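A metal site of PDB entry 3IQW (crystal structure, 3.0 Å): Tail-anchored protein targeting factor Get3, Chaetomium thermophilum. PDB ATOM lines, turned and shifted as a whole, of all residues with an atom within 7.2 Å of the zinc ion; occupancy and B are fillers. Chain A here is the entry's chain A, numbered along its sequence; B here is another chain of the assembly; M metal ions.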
ATOM      1  N   LEU A 262      14.941 -20.993  39.199  1.00  0.00           N
ATOM      2  CA  LEU A 262      15.579 -21.096  37.902  1.00  0.00           C
ATOM      3  C   LEU A 262      16.921 -20.398  38.027  1.00  0.00           C
ATOM      4  O   LEU A 262      16.965 -19.211  38.273  1.00  0.00           O
ATOM      5  CB  LEU A 262      14.704 -20.401  36.855  1.00  0.00           C
ATOM      6  CG  LEU A 262      14.733 -20.716  35.358  1.00  0.00           C
ATOM      7  CD1 LEU A 262      15.762 -19.863  34.651  1.00  0.00           C
ATOM      8  CD2 LEU A 262      14.974 -22.181  35.086  1.00  0.00           C
ATOM      9  N   PRO A 264      19.659 -19.500  35.556  1.00  0.00           N
ATOM     10  CA  PRO A 264      20.113 -19.708  34.172  1.00  0.00           C
ATOM     11  C   PRO A 264      21.538 -20.240  34.161  1.00  0.00           C
ATOM     12  O   PRO A 264      22.312 -19.986  35.098  1.00  0.00           O
ATOM     13  CB  PRO A 264      20.103 -18.295  33.570  1.00  0.00           C
ATOM     14  CG  PRO A 264      19.347 -17.445  34.528  1.00  0.00           C
ATOM     15  CD  PRO A 264      19.407 -18.084  35.866  1.00  0.00           C
ATOM     16  N   SER A 268      25.000 -18.356  29.215  1.00  0.00           N
ATOM     17  CA  SER A 268      23.812 -18.641  28.427  1.00  0.00           C
ATOM     18  C   SER A 268      22.943 -17.400  28.499  1.00  0.00           C
ATOM     19  O   SER A 268      22.454 -17.043  29.586  1.00  0.00           O
ATOM     20  CB  SER A 268      22.993 -19.808  29.056  1.00  0.00           C
ATOM     21  OG  SER A 268      23.698 -21.065  29.077  1.00  0.00           O
ATOM     22  N   ASP A 269      22.723 -16.754  27.357  1.00  0.00           N
ATOM     23  CA  ASP A 269      21.816 -15.639  27.348  1.00  0.00           C
ATOM     24  C   ASP A 269      20.475 -16.107  26.786  1.00  0.00           C
ATOM     25  O   ASP A 269      20.408 -16.643  25.684  1.00  0.00           O
ATOM     26  CB  ASP A 269      22.366 -14.611  26.433  1.00  0.00           C
ATOM     27  CG  ASP A 269      22.310 -15.085  25.026  1.00  0.00           C
ATOM     28  OD1 ASP A 269      21.311 -15.874  24.736  1.00  0.00           O
ATOM     29  OD2 ASP A 269      23.261 -14.771  24.211  1.00  0.00           O
ATOM     30  N   CYS A 270      19.413 -15.899  27.559  1.00  0.00           N
ATOM     31  CA  CYS A 270      18.083 -16.287  27.195  1.00  0.00           C
ATOM     32  C   CYS A 270      17.184 -15.129  27.610  1.00  0.00           C
ATOM     33  O   CYS A 270      17.239 -14.716  28.758  1.00  0.00           O
ATOM     34  CB  CYS A 270      17.687 -17.496  28.015  1.00  0.00           C
ATOM     35  SG  CYS A 270      16.401 -18.377  27.329  1.00  0.00           S
ATOM     36  N   GLU A 271      16.368 -14.588  26.713  1.00  0.00           N
ATOM     37  CA  GLU A 271      15.265 -13.757  27.174  1.00  0.00           C
ATOM     38  C   GLU A 271      14.559 -14.390  28.410  1.00  0.00           C
ATOM     39  O   GLU A 271      14.667 -13.909  29.539  1.00  0.00           O
ATOM     40  CB  GLU A 271      14.235 -13.729  26.054  1.00  0.00           C
ATOM     41  CG  GLU A 271      14.973 -13.662  24.688  1.00  0.00           C
ATOM     42  CD  GLU A 271      15.017 -12.186  24.291  1.00  0.00           C
ATOM     43  OE1 GLU A 271      14.617 -11.627  25.301  1.00  0.00           O
ATOM     44  OE2 GLU A 271      15.660 -11.581  23.456  1.00  0.00           O
ATOM     45  N   GLN A 272      13.814 -15.454  28.166  1.00  0.00           N
ATOM     46  CA  GLN A 272      12.928 -15.981  29.163  1.00  0.00           C
ATOM     47  C   GLN A 272      13.770 -16.306  30.357  1.00  0.00           C
ATOM     48  O   GLN A 272      13.618 -15.738  31.439  1.00  0.00           O
ATOM     49  CB  GLN A 272      12.265 -17.266  28.662  1.00  0.00           C
ATOM     50  CG  GLN A 272      11.174 -17.098  27.625  1.00  0.00           C
ATOM     51  CD  GLN A 272      10.321 -18.330  27.516  1.00  0.00           C
ATOM     52  OE1 GLN A 272       9.725 -18.794  28.498  1.00  0.00           O
ATOM     53  NE2 GLN A 272      10.258 -18.893  26.306  1.00  0.00           N
ATOM     54  N   CYS A 273      14.659 -17.270  30.174  1.00  0.00           N
ATOM     55  CA  CYS A 273      15.526 -17.652  31.235  1.00  0.00           C
ATOM     56  C   CYS A 273      16.012 -16.445  32.035  1.00  0.00           C
ATOM     57  O   CYS A 273      15.880 -16.410  33.250  1.00  0.00           O
ATOM     58  CB  CYS A 273      16.689 -18.439  30.681  1.00  0.00           C
ATOM     59  SG  CYS A 273      16.290 -20.076  30.909  1.00  0.00           S
ATOM     60  N   THR A 274      16.559 -15.447  31.368  1.00  0.00           N
ATOM     61  CA  THR A 274      17.089 -14.312  32.102  1.00  0.00           C
ATOM     62  C   THR A 274      16.016 -13.616  32.919  1.00  0.00           C
ATOM     63  O   THR A 274      16.111 -13.520  34.142  1.00  0.00           O
ATOM     64  CB  THR A 274      17.713 -13.284  31.194  1.00  0.00           C
ATOM     65  OG1 THR A 274      18.901 -13.824  30.645  1.00  0.00           O
ATOM     66  CG2 THR A 274      18.087 -12.077  31.984  1.00  0.00           C
ATOM     67  N   LEU B 262       5.909 -24.117  28.641  1.00  0.00           N
ATOM     68  CA  LEU B 262       7.048 -23.324  28.269  1.00  0.00           C
ATOM     69  C   LEU B 262       7.198 -23.521  26.767  1.00  0.00           C
ATOM     70  O   LEU B 262       7.415 -24.640  26.298  1.00  0.00           O
ATOM     71  CB  LEU B 262       8.278 -23.814  29.024  1.00  0.00           C
ATOM     72  CG  LEU B 262       9.587 -23.025  29.156  1.00  0.00           C
ATOM     73  CD1 LEU B 262      10.519 -23.196  27.937  1.00  0.00           C
ATOM     74  CD2 LEU B 262       9.342 -21.556  29.473  1.00  0.00           C
ATOM     75  N   PRO B 264       9.795 -22.522  24.133  1.00  0.00           N
ATOM     76  CA  PRO B 264      11.004 -21.746  23.903  1.00  0.00           C
ATOM     77  C   PRO B 264      10.763 -20.767  22.774  1.00  0.00           C
ATOM     78  O   PRO B 264       9.894 -20.996  21.930  1.00  0.00           O
ATOM     79  CB  PRO B 264      12.018 -22.783  23.431  1.00  0.00           C
ATOM     80  CG  PRO B 264      11.450 -24.095  23.797  1.00  0.00           C
ATOM     81  CD  PRO B 264       9.973 -23.956  23.842  1.00  0.00           C
ATOM     82  N   SER B 268      15.952 -19.673  19.348  1.00  0.00           N
ATOM     83  CA  SER B 268      16.621 -19.535  20.664  1.00  0.00           C
ATOM     84  C   SER B 268      17.006 -20.924  21.091  1.00  0.00           C
ATOM     85  O   SER B 268      16.144 -21.787  21.286  1.00  0.00           O
ATOM     86  CB  SER B 268      15.674 -18.943  21.700  1.00  0.00           C
ATOM     87  OG  SER B 268      15.185 -17.674  21.295  1.00  0.00           O
ATOM     88  N   ASP B 269      18.301 -21.159  21.233  1.00  0.00           N
ATOM     89  CA  ASP B 269      18.756 -22.437  21.717  1.00  0.00           C
ATOM     90  C   ASP B 269      19.112 -22.286  23.198  1.00  0.00           C
ATOM     91  O   ASP B 269      19.971 -21.474  23.558  1.00  0.00           O
ATOM     92  CB  ASP B 269      19.977 -22.838  20.942  1.00  0.00           C
ATOM     93  CG  ASP B 269      21.130 -21.934  21.253  1.00  0.00           C
ATOM     94  OD1 ASP B 269      21.140 -21.364  22.411  1.00  0.00           O
ATOM     95  OD2 ASP B 269      21.974 -21.689  20.348  1.00  0.00           O
ATOM     96  N   CYS B 270      18.455 -23.074  24.036  1.00  0.00           N
ATOM     97  CA  CYS B 270      18.691 -23.063  25.459  1.00  0.00           C
ATOM     98  C   CYS B 270      18.705 -24.490  25.905  1.00  0.00           C
ATOM     99  O   CYS B 270      17.805 -25.249  25.583  1.00  0.00           O
ATOM    100  CB  CYS B 270      17.503 -22.405  26.124  1.00  0.00           C
ATOM    101  SG  CYS B 270      17.917 -21.515  27.572  1.00  0.00           S
ATOM    102  N   GLU B 271      19.672 -24.906  26.686  1.00  0.00           N
ATOM    103  CA  GLU B 271      19.517 -26.263  27.126  1.00  0.00           C
ATOM    104  C   GLU B 271      18.280 -26.426  27.955  1.00  0.00           C
ATOM    105  O   GLU B 271      17.394 -27.215  27.619  1.00  0.00           O
ATOM    106  CB  GLU B 271      20.716 -26.738  27.903  1.00  0.00           C
ATOM    107  CG  GLU B 271      21.807 -27.085  26.871  1.00  0.00           C
ATOM    108  CD  GLU B 271      23.075 -26.631  27.325  1.00  0.00           C
ATOM    109  OE1 GLU B 271      22.976 -26.247  28.547  1.00  0.00           O
ATOM    110  OE2 GLU B 271      24.189 -26.745  26.682  1.00  0.00           O
ATOM    111  N   GLN B 272      18.197 -25.662  29.038  1.00  0.00           N
ATOM    112  CA  GLN B 272      17.061 -25.813  29.959  1.00  0.00           C
ATOM    113  C   GLN B 272      15.801 -25.612  29.183  1.00  0.00           C
ATOM    114  O   GLN B 272      14.955 -26.496  29.108  1.00  0.00           O
ATOM    115  CB  GLN B 272      17.089 -24.761  31.056  1.00  0.00           C
ATOM    116  CG  GLN B 272      18.166 -24.954  32.087  1.00  0.00           C
ATOM    117  CD  GLN B 272      17.851 -24.135  33.301  1.00  0.00           C
ATOM    118  OE1 GLN B 272      16.850 -24.357  33.954  1.00  0.00           O
ATOM    119  NE2 GLN B 272      18.695 -23.165  33.590  1.00  0.00           N
ATOM    120  N   CYS B 273      15.647 -24.423  28.639  1.00  0.00           N
ATOM    121  CA  CYS B 273      14.492 -24.135  27.830  1.00  0.00           C
ATOM    122  C   CYS B 273      14.131 -25.273  26.856  1.00  0.00           C
ATOM    123  O   CYS B 273      12.998 -25.756  26.850  1.00  0.00           O
ATOM    124  CB  CYS B 273      14.706 -22.831  27.090  1.00  0.00           C
ATOM    125  SG  CYS B 273      13.964 -21.492  27.969  1.00  0.00           S
ATOM    126  N   THR B 274      15.091 -25.724  26.061  1.00  0.00           N
ATOM    127  CA  THR B 274      14.800 -26.805  25.126  1.00  0.00           C
ATOM    128  C   THR B 274      14.354 -28.057  25.844  1.00  0.00           C
ATOM    129  O   THR B 274      13.249 -28.541  25.606  1.00  0.00           O
ATOM    130  CB  THR B 274      16.014 -27.185  24.272  1.00  0.00           C
ATOM    131  OG1 THR B 274      16.345 -26.094  23.413  1.00  0.00           O
ATOM    132  CG2 THR B 274      15.684 -28.391  23.409  1.00  0.00           C
ATOM    133  N   ARG B 276      13.246 -28.581  28.549  1.00  0.00           N
ATOM    134  CA  ARG B 276      12.058 -28.426  29.318  1.00  0.00           C
ATOM    135  C   ARG B 276      10.850 -28.610  28.461  1.00  0.00           C
ATOM    136  O   ARG B 276       9.868 -29.250  28.845  1.00  0.00           O
ATOM    137  CB  ARG B 276      12.020 -27.045  29.886  1.00  0.00           C
ATOM    138  CG  ARG B 276      11.373 -27.030  31.219  1.00  0.00           C
ATOM    139  CD  ARG B 276      12.138 -26.045  32.026  1.00  0.00           C
ATOM    140  NE  ARG B 276      11.433 -25.442  33.146  1.00  0.00           N
ATOM    141  CZ  ARG B 276      11.694 -24.221  33.597  1.00  0.00           C
ATOM    142  NH1 ARG B 276      12.592 -23.453  33.038  1.00  0.00           N
ATOM    143  NH2 ARG B 276      11.021 -23.701  34.573  1.00  0.00           N
HETATM  144 ZN    ZN M   1      15.970 -20.250  28.474  1.00  0.00          ZN
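The side-chain hydroxyl of Thr 274 of chain A is in hydrogen-bond range of the backbone carbonyl oxygen of Cys 270 of chain A (2.7 Å).
The backbone carbonyl oxygen (O) of Cys 270 of chain B is in hydrogen-bond range of the side-chain hydroxyl (OG1) of Thr 274 of chain B (2.7 Å).
Of the 19 residues printed, 4 come within 4 Å of the zinc ion.
The nearest printed residue that does not touch the zinc ion is Gln 272 of chain A (4.8 Å).
The zinc ion is bound by SG of Cys 270 of chain A (2.2 Å), SG of Cys 273 of chain B (2.4 Å), SG of Cys 273 of chain A (2.5 Å) and SG of Cys 270 of chain B (2.5 Å).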
